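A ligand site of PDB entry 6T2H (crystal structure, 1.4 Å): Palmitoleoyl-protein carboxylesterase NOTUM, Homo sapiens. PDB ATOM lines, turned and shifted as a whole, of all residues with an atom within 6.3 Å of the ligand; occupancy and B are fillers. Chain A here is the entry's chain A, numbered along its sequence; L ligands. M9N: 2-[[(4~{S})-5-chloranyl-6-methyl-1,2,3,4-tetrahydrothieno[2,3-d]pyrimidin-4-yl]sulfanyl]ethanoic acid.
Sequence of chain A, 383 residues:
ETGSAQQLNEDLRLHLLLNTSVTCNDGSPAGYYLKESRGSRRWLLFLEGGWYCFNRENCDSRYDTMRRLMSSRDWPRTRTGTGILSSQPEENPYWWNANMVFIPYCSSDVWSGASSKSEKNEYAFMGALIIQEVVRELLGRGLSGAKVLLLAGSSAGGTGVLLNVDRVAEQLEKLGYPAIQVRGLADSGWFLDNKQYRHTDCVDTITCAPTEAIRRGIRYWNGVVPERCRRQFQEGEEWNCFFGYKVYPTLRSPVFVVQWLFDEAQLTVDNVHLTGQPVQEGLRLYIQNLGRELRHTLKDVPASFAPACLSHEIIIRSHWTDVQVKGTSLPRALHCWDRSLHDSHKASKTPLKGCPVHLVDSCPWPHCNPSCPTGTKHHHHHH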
ATOM      1  N   GLY A  49      16.378 -32.327 -15.156  1.00  0.00           N
ATOM      2  CA  GLY A  49      16.360 -32.133 -16.603  1.00  0.00           C
ATOM      3  C   GLY A  49      17.753 -32.220 -17.217  1.00  0.00           C
ATOM      4  O   GLY A  49      18.728 -32.633 -16.583  1.00  0.00           O
ATOM      5  N   GLY A  50      17.816 -31.812 -18.477  1.00  0.00           N
ATOM      6  CA  GLY A  50      19.075 -31.825 -19.210  1.00  0.00           C
ATOM      7  C   GLY A  50      18.973 -32.326 -20.630  1.00  0.00           C
ATOM      8  O   GLY A  50      19.806 -33.161 -21.038  1.00  0.00           O
ATOM      9  N   TRP A  51      18.024 -31.850 -21.398  1.00  0.00           N
ATOM     10  CA  TRP A  51      17.897 -32.162 -22.849  1.00  0.00           C
ATOM     11  C   TRP A  51      17.672 -33.668 -23.000  1.00  0.00           C
ATOM     12  O   TRP A  51      16.923 -34.252 -22.193  1.00  0.00           O
ATOM     13  CB  TRP A  51      19.019 -31.574 -23.679  1.00  0.00           C
ATOM     14  CG  TRP A  51      18.992 -30.077 -23.665  1.00  0.00           C
ATOM     15  CD1 TRP A  51      19.717 -29.264 -22.865  1.00  0.00           C
ATOM     16  CD2 TRP A  51      18.246 -29.236 -24.546  1.00  0.00           C
ATOM     17  NE1 TRP A  51      19.466 -27.933 -23.177  1.00  0.00           N
ATOM     18  CE2 TRP A  51      18.558 -27.894 -24.200  1.00  0.00           C
ATOM     19  CE3 TRP A  51      17.337 -29.471 -25.566  1.00  0.00           C
ATOM     20  CZ2 TRP A  51      17.984 -26.808 -24.865  1.00  0.00           C
ATOM     21  CZ3 TRP A  51      16.781 -28.390 -26.229  1.00  0.00           C
ATOM     22  CH2 TRP A  51      17.120 -27.077 -25.869  1.00  0.00           C
ATOM     23  N   TYR A  52      18.264 -34.294 -24.023  1.00  0.00           N
ATOM     24  CA  TYR A  52      17.997 -35.681 -24.377  1.00  0.00           C
ATOM     25  C   TYR A  52      18.950 -35.988 -25.525  1.00  0.00           C
ATOM     26  O   TYR A  52      19.619 -35.100 -26.043  1.00  0.00           O
ATOM     27  CB  TYR A  52      16.546 -35.917 -24.820  1.00  0.00           C
ATOM     28  CG  TYR A  52      16.032 -34.925 -25.816  1.00  0.00           C
ATOM     29  CD1 TYR A  52      16.335 -35.082 -27.159  1.00  0.00           C
ATOM     30  CD2 TYR A  52      15.264 -33.828 -25.418  1.00  0.00           C
ATOM     31  CE1 TYR A  52      15.890 -34.153 -28.098  1.00  0.00           C
ATOM     32  CE2 TYR A  52      14.816 -32.906 -26.346  1.00  0.00           C
ATOM     33  CZ  TYR A  52      15.132 -33.080 -27.688  1.00  0.00           C
ATOM     34  OH  TYR A  52      14.712 -32.178 -28.629  1.00  0.00           O
ATOM     35  N   TYR A 105      18.682 -37.517 -13.678  1.00  0.00           N
ATOM     36  CA  TYR A 105      18.296 -37.812 -15.043  1.00  0.00           C
ATOM     37  C   TYR A 105      19.496 -38.485 -15.703  1.00  0.00           C
ATOM     38  O   TYR A 105      20.484 -37.832 -16.008  1.00  0.00           O
ATOM     39  CB  TYR A 105      17.998 -36.478 -15.713  1.00  0.00           C
ATOM     40  CG  TYR A 105      17.527 -36.518 -17.143  1.00  0.00           C
ATOM     41  CD1 TYR A 105      16.637 -37.499 -17.612  1.00  0.00           C
ATOM     42  CD2 TYR A 105      17.916 -35.506 -18.030  1.00  0.00           C
ATOM     43  CE1 TYR A 105      16.181 -37.492 -18.939  1.00  0.00           C
ATOM     44  CE2 TYR A 105      17.431 -35.473 -19.330  1.00  0.00           C
ATOM     45  CZ  TYR A 105      16.599 -36.481 -19.784  1.00  0.00           C
ATOM     46  OH  TYR A 105      16.145 -36.470 -21.081  1.00  0.00           O
ATOM     47  N   VAL A 110      13.793 -37.872 -21.902  1.00  0.00           N
ATOM     48  CA  VAL A 110      12.699 -37.059 -21.364  1.00  0.00           C
ATOM     49  C   VAL A 110      11.854 -37.904 -20.399  1.00  0.00           C
ATOM     50  O   VAL A 110      10.644 -37.673 -20.246  1.00  0.00           O
ATOM     51  CB  VAL A 110      11.860 -36.369 -22.464  1.00  0.00           C
ATOM     52  CG1 VAL A 110      11.057 -35.178 -21.877  1.00  0.00           C
ATOM     53  CG2 VAL A 110      12.782 -35.874 -23.593  1.00  0.00           C
ATOM     54  N   SER A 154      12.166 -30.185 -13.483  1.00  0.00           N
ATOM     55  CA  SER A 154      12.517 -28.987 -14.234  1.00  0.00           C
ATOM     56  C   SER A 154      13.047 -29.332 -15.620  1.00  0.00           C
ATOM     57  O   SER A 154      13.796 -30.321 -15.788  1.00  0.00           O
ATOM     58  CB  SER A 154      13.601 -28.191 -13.510  1.00  0.00           C
ATOM     59  OG  SER A 154      13.114 -27.594 -12.304  1.00  0.00           O
ATOM     60  N   SER A 155      12.637 -28.522 -16.610  1.00  0.00           N
ATOM     61  CA  SER A 155      13.152 -28.638 -18.007  1.00  0.00           C
ATOM     62  C   SER A 155      12.696 -29.983 -18.567  1.00  0.00           C
ATOM     63  O   SER A 155      11.498 -30.282 -18.523  1.00  0.00           O
ATOM     64  CB  SER A 155      14.648 -28.403 -18.028  1.00  0.00           C
ATOM     65  OG  SER A 155      14.948 -27.209 -17.349  1.00  0.00           O
ATOM     66  N   ALA A 156      13.610 -30.834 -19.076  1.00  0.00           N
ATOM     67  CA  ALA A 156      13.142 -32.158 -19.513  1.00  0.00           C
ATOM     68  C   ALA A 156      12.472 -32.909 -18.369  1.00  0.00           C
ATOM     69  O   ALA A 156      11.613 -33.769 -18.604  1.00  0.00           O
ATOM     70  CB  ALA A 156      14.320 -32.986 -20.081  1.00  0.00           C
ATOM     71  N   GLY A 157      12.859 -32.620 -17.112  1.00  0.00           N
ATOM     72  CA  GLY A 157      12.168 -33.234 -15.988  1.00  0.00           C
ATOM     73  C   GLY A 157      10.764 -32.714 -15.787  1.00  0.00           C
ATOM     74  O   GLY A 157       9.883 -33.447 -15.305  1.00  0.00           O
ATOM     75  N   THR A 159       8.779 -31.803 -18.370  1.00  0.00           N
ATOM     76  CA  THR A 159       8.029 -32.613 -19.331  1.00  0.00           C
ATOM     77  C   THR A 159       7.858 -34.032 -18.812  1.00  0.00           C
ATOM     78  O   THR A 159       6.783 -34.636 -18.976  1.00  0.00           O
ATOM     79  CB  THR A 159       8.754 -32.617 -20.683  1.00  0.00           C
ATOM     80  OG1 THR A 159       9.096 -31.259 -21.064  1.00  0.00           O
ATOM     81  CG2 THR A 159       7.885 -33.242 -21.747  1.00  0.00           C
ATOM     82  N   SER A 188       9.257 -25.402 -16.339  1.00  0.00           N
ATOM     83  CA  SER A 188      10.083 -25.201 -17.538  1.00  0.00           C
ATOM     84  C   SER A 188      10.026 -26.386 -18.499  1.00  0.00           C
ATOM     85  O   SER A 188      10.986 -26.617 -19.266  1.00  0.00           O
ATOM     86  CB  SER A 188      11.516 -24.892 -17.147  1.00  0.00           C
ATOM     87  OG  SER A 188      11.524 -23.699 -16.342  1.00  0.00           O
ATOM     88  N   GLY A 189       8.917 -27.127 -18.501  1.00  0.00           N
ATOM     89  CA  GLY A 189       8.767 -28.255 -19.390  1.00  0.00           C
ATOM     90  C   GLY A 189       7.575 -28.137 -20.302  1.00  0.00           C
ATOM     91  O   GLY A 189       7.105 -29.155 -20.844  1.00  0.00           O
ATOM     92  N   PHE A 191       6.451 -26.702 -23.595  1.00  0.00           N
ATOM     93  CA  PHE A 191       7.037 -26.208 -24.843  1.00  0.00           C
ATOM     94  C   PHE A 191       6.001 -26.093 -25.939  1.00  0.00           C
ATOM     95  O   PHE A 191       4.952 -26.739 -25.924  1.00  0.00           O
ATOM     96  CB  PHE A 191       8.168 -27.152 -25.292  1.00  0.00           C
ATOM     97  CG  PHE A 191       9.296 -27.206 -24.295  1.00  0.00           C
ATOM     98  CD1 PHE A 191       9.475 -28.309 -23.474  1.00  0.00           C
ATOM     99  CD2 PHE A 191      10.098 -26.104 -24.125  1.00  0.00           C
ATOM    100  CE1 PHE A 191      10.537 -28.346 -22.527  1.00  0.00           C
ATOM    101  CE2 PHE A 191      11.140 -26.122 -23.172  1.00  0.00           C
ATOM    102  CZ  PHE A 191      11.346 -27.257 -22.390  1.00  0.00           C
ATOM    103  N   LEU A 192       6.306 -25.250 -26.926  1.00  0.00           N
ATOM    104  CA  LEU A 192       5.441 -25.065 -28.076  1.00  0.00           C
ATOM    105  C   LEU A 192       6.131 -25.644 -29.302  1.00  0.00           C
ATOM    106  O   LEU A 192       7.328 -25.374 -29.522  1.00  0.00           O
ATOM    107  CB  LEU A 192       5.204 -23.575 -28.324  1.00  0.00           C
ATOM    108  CG  LEU A 192       4.516 -22.791 -27.216  1.00  0.00           C
ATOM    109  CD1 LEU A 192       4.286 -21.379 -27.694  1.00  0.00           C
ATOM    110  CD2 LEU A 192       3.197 -23.478 -26.816  1.00  0.00           C
ATOM    111  N   PRO A 210      12.466 -29.928 -32.326  1.00  0.00           N
ATOM    112  CA  PRO A 210      12.067 -30.886 -31.277  1.00  0.00           C
ATOM    113  C   PRO A 210      11.018 -31.878 -31.729  1.00  0.00           C
ATOM    114  O   PRO A 210      11.114 -33.065 -31.358  1.00  0.00           O
ATOM    115  CB  PRO A 210      11.565 -29.976 -30.147  1.00  0.00           C
ATOM    116  CG  PRO A 210      12.284 -28.695 -30.361  1.00  0.00           C
ATOM    117  CD  PRO A 210      12.408 -28.534 -31.851  1.00  0.00           C
ATOM    118  N   THR A 211      10.042 -31.472 -32.541  1.00  0.00           N
ATOM    119  CA  THR A 211       9.055 -32.433 -33.007  1.00  0.00           C
ATOM    120  C   THR A 211       9.716 -33.597 -33.729  1.00  0.00           C
ATOM    121  O   THR A 211       9.422 -34.763 -33.435  1.00  0.00           O
ATOM    122  CB  THR A 211       7.962 -31.803 -33.870  1.00  0.00           C
ATOM    123  OG1 THR A 211       8.537 -31.268 -35.052  1.00  0.00           O
ATOM    124  CG2 THR A 211       7.257 -30.689 -33.116  1.00  0.00           C
ATOM    125  N   ILE A 214      12.080 -35.560 -31.198  1.00  0.00           N
ATOM    126  CA  ILE A 214      11.242 -36.384 -30.338  1.00  0.00           C
ATOM    127  C   ILE A 214      10.611 -37.538 -31.109  1.00  0.00           C
ATOM    128  O   ILE A 214      10.544 -38.665 -30.623  1.00  0.00           O
ATOM    129  CB  ILE A 214      10.188 -35.521 -29.619  1.00  0.00           C
ATOM    130  CG1 ILE A 214      10.848 -34.519 -28.653  1.00  0.00           C
ATOM    131  CG2 ILE A 214       9.233 -36.415 -28.845  1.00  0.00           C
ATOM    132  CD1 ILE A 214      11.542 -35.194 -27.470  1.00  0.00           C
ATOM    133  N   PHE A 242       4.459 -35.030 -25.872  1.00  0.00           N
ATOM    134  CA  PHE A 242       5.567 -34.365 -25.192  1.00  0.00           C
ATOM    135  C   PHE A 242       5.362 -32.867 -25.097  1.00  0.00           C
ATOM    136  O   PHE A 242       6.201 -32.183 -24.505  1.00  0.00           O
ATOM    137  CB  PHE A 242       6.876 -34.671 -25.929  1.00  0.00           C
ATOM    138  CG  PHE A 242       7.407 -36.053 -25.694  1.00  0.00           C
ATOM    139  CD1 PHE A 242       6.712 -37.179 -26.118  1.00  0.00           C
ATOM    140  CD2 PHE A 242       8.674 -36.241 -25.101  1.00  0.00           C
ATOM    141  CE1 PHE A 242       7.237 -38.467 -25.953  1.00  0.00           C
ATOM    142  CE2 PHE A 242       9.193 -37.528 -24.929  1.00  0.00           C
ATOM    143  CZ  PHE A 242       8.480 -38.622 -25.346  1.00  0.00           C
ATOM    144  N   PHE A 243       4.281 -32.358 -25.663  1.00  0.00           N
ATOM    145  CA  PHE A 243       3.992 -30.928 -25.678  1.00  0.00           C
ATOM    146  C   PHE A 243       2.893 -30.673 -24.673  1.00  0.00           C
ATOM    147  O   PHE A 243       1.760 -31.157 -24.835  1.00  0.00           O
ATOM    148  CB  PHE A 243       3.662 -30.483 -27.100  1.00  0.00           C
ATOM    149  CG  PHE A 243       4.892 -30.481 -27.944  1.00  0.00           C
ATOM    150  CD1 PHE A 243       5.284 -31.632 -28.602  1.00  0.00           C
ATOM    151  CD2 PHE A 243       5.755 -29.405 -27.879  1.00  0.00           C
ATOM    152  CE1 PHE A 243       6.466 -31.669 -29.294  1.00  0.00           C
ATOM    153  CE2 PHE A 243       6.951 -29.428 -28.601  1.00  0.00           C
ATOM    154  CZ  PHE A 243       7.296 -30.560 -29.278  1.00  0.00           C
ATOM    155  N   ASP A 263      11.009 -18.706 -22.364  1.00  0.00           N
ATOM    156  CA  ASP A 263      11.960 -19.677 -21.841  1.00  0.00           C
ATOM    157  C   ASP A 263      13.174 -19.796 -22.768  1.00  0.00           C
ATOM    158  O   ASP A 263      13.051 -19.917 -23.990  1.00  0.00           O
ATOM    159  CB  ASP A 263      11.233 -21.012 -21.750  1.00  0.00           C
ATOM    160  CG  ASP A 263      12.097 -22.078 -21.174  1.00  0.00           C
ATOM    161  OD1 ASP A 263      12.185 -22.190 -19.932  1.00  0.00           O
ATOM    162  OD2 ASP A 263      12.694 -22.802 -21.991  1.00  0.00           O
ATOM    163  N   ALA A 265      15.244 -22.259 -23.313  1.00  0.00           N
ATOM    164  CA  ALA A 265      15.343 -23.482 -24.125  1.00  0.00           C
ATOM    165  C   ALA A 265      14.376 -23.425 -25.300  1.00  0.00           C
ATOM    166  O   ALA A 265      14.694 -23.902 -26.389  1.00  0.00           O
ATOM    167  CB  ALA A 265      15.082 -24.709 -23.246  1.00  0.00           C
ATOM    168  N   GLN A 266      13.178 -22.860 -25.092  1.00  0.00           N
ATOM    169  CA  GLN A 266      12.248 -22.643 -26.196  1.00  0.00           C
ATOM    170  C   GLN A 266      12.868 -21.725 -27.228  1.00  0.00           C
ATOM    171  O   GLN A 266      12.847 -21.999 -28.435  1.00  0.00           O
ATOM    172  CB  GLN A 266      10.954 -22.029 -25.644  1.00  0.00           C
ATOM    173  CG  GLN A 266       9.930 -21.679 -26.714  1.00  0.00           C
ATOM    174  CD  GLN A 266       9.191 -22.884 -27.210  1.00  0.00           C
ATOM    175  OE1 GLN A 266       8.660 -23.679 -26.411  1.00  0.00           O
ATOM    176  NE2 GLN A 266       9.148 -23.048 -28.559  1.00  0.00           N
ATOM    177  N   VAL A 269      15.639 -23.654 -29.275  1.00  0.00           N
ATOM    178  CA  VAL A 269      15.102 -24.501 -30.322  1.00  0.00           C
ATOM    179  C   VAL A 269      14.439 -23.687 -31.423  1.00  0.00           C
ATOM    180  O   VAL A 269      14.373 -24.153 -32.568  1.00  0.00           O
ATOM    181  CB  VAL A 269      14.190 -25.622 -29.798  1.00  0.00           C
ATOM    182  CG1 VAL A 269      14.944 -26.522 -28.849  1.00  0.00           C
ATOM    183  CG2 VAL A 269      12.940 -25.068 -29.143  1.00  0.00           C
ATOM    184  N   HIS A 312      15.451 -19.699 -17.455  1.00  0.00           N
ATOM    185  CA  HIS A 312      15.321 -21.136 -17.622  1.00  0.00           C
ATOM    186  C   HIS A 312      15.367 -21.835 -16.271  1.00  0.00           C
ATOM    187  O   HIS A 312      16.323 -21.630 -15.517  1.00  0.00           O
ATOM    188  CB  HIS A 312      16.462 -21.686 -18.487  1.00  0.00           C
ATOM    189  CG  HIS A 312      16.307 -23.136 -18.798  1.00  0.00           C
ATOM    190  ND1 HIS A 312      17.290 -24.064 -18.523  1.00  0.00           N
ATOM    191  CD2 HIS A 312      15.282 -23.822 -19.330  1.00  0.00           C
ATOM    192  CE1 HIS A 312      16.877 -25.259 -18.897  1.00  0.00           C
ATOM    193  NE2 HIS A 312      15.657 -25.147 -19.396  1.00  0.00           N
ATOM    194  N   GLU A 313      14.362 -22.692 -15.999  1.00  0.00           N
ATOM    195  CA  GLU A 313      14.115 -23.376 -14.702  1.00  0.00           C
ATOM    196  C   GLU A 313      13.837 -22.380 -13.594  1.00  0.00           C
ATOM    197  O   GLU A 313      14.175 -21.208 -13.724  1.00  0.00           O
ATOM    198  CB  GLU A 313      15.262 -24.291 -14.304  1.00  0.00           C
ATOM    199  CG  GLU A 313      15.289 -25.545 -15.070  1.00  0.00           C
ATOM    200  CD  GLU A 313      16.565 -26.354 -14.879  1.00  0.00           C
ATOM    201  OE1 GLU A 313      17.384 -25.987 -13.997  1.00  0.00           O
ATOM    202  OE2 GLU A 313      16.746 -27.362 -15.598  1.00  0.00           O
HETATM  203  C10 M9N L   1      10.641 -30.992 -25.530  1.00  0.00           C
HETATM  204  C13 M9N L   1      11.973 -28.913 -25.989  1.00  0.00           C
HETATM  205  C15 M9N L   1      13.657 -27.114 -25.668  1.00  0.00           C
HETATM  206  C01 M9N L   1      13.820 -29.102 -24.352  1.00  0.00           C
HETATM  207  C03 M9N L   1      15.526 -28.503 -22.250  1.00  0.00           C
HETATM  208  C04 M9N L   1      16.296 -28.866 -20.991  1.00  0.00           C
HETATM  209  C07 M9N L   1      12.507 -29.637 -24.936  1.00  0.00           C
HETATM  210  C08 M9N L   1      11.768 -30.858 -24.705  1.00  0.00           C
HETATM  211  C11 M9N L   1       9.658 -32.148 -25.464  1.00  0.00           C
HETATM  212  N14 M9N L   1      12.553 -27.691 -26.367  1.00  0.00           N
HETATM  213  N16 M9N L   1      13.911 -27.637 -24.335  1.00  0.00           N
HETATM  214  O05 M9N L   1      17.059 -28.008 -20.489  1.00  0.00           O
HETATM  215  O06 M9N L   1      16.163 -29.974 -20.389  1.00  0.00           O
HETATM  216  S02 M9N L   1      14.361 -29.798 -22.776  1.00  0.00           S
HETATM  217  S12 M9N L   1      10.597 -29.671 -26.605  1.00  0.00           S
HETATM  218 CL1  M9N L   1      12.148 -32.040 -23.429  1.00  0.00          CL
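An oxygen (O06) of the ligand sits at hydrogen-bond distance from the backbone NH (N) of Ala 156. O05 of the ligand sits close to NE2 of His 312 (3.4 Å). The backbone NH of Gly 50 is in hydrogen-bond range of an oxygen (O06) of the ligand, at 3.1 Å. An oxygen (O06) of the ligand is in hydrogen-bond range of the backbone NH (N) of Trp 51 (2.8 Å).
The backbone carbonyl oxygen (O) of Trp 51 lies within hydrogen-bond range of the side-chain hydroxyl (OH) of Tyr 105 (2.6 Å). The side-chain carboxylate of Asp 263 sits at hydrogen-bond distance from the backbone NH of Ala 265. OG of Ser 155 is in hydrogen-bond range of OE2 of Glu 313, 2.5 Å away. N of Val 110 is in hydrogen-bond range of OH of Tyr 105. The side-chain hydroxyl (OG) of Ser 155 lies within hydrogen-bond range of a ring nitrogen (NE2) of His 312 (3.0 Å). OG1 of Thr 159 sits at hydrogen-bond distance from O of Gly 189 (2.9 Å).
Val 110 touches the ligand. CB of Ser 155 touches O06 of the ligand, 3.2 Å away. OG1 of Thr 159 touches CL1 of the ligand, at 3.9 Å. Phe 191 touches the ligand. Pro 210 touches the ligand. O of Phe 242 touches C11 of the ligand, 3.6 Å away. Ala 265 touches the ligand. Val 269 touches the ligand. Along chain A the residues within 4 Å of the ligand span positions 50 to 312. The nearest printed residue that does not touch the ligand is Tyr 52 (4.02 Å).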
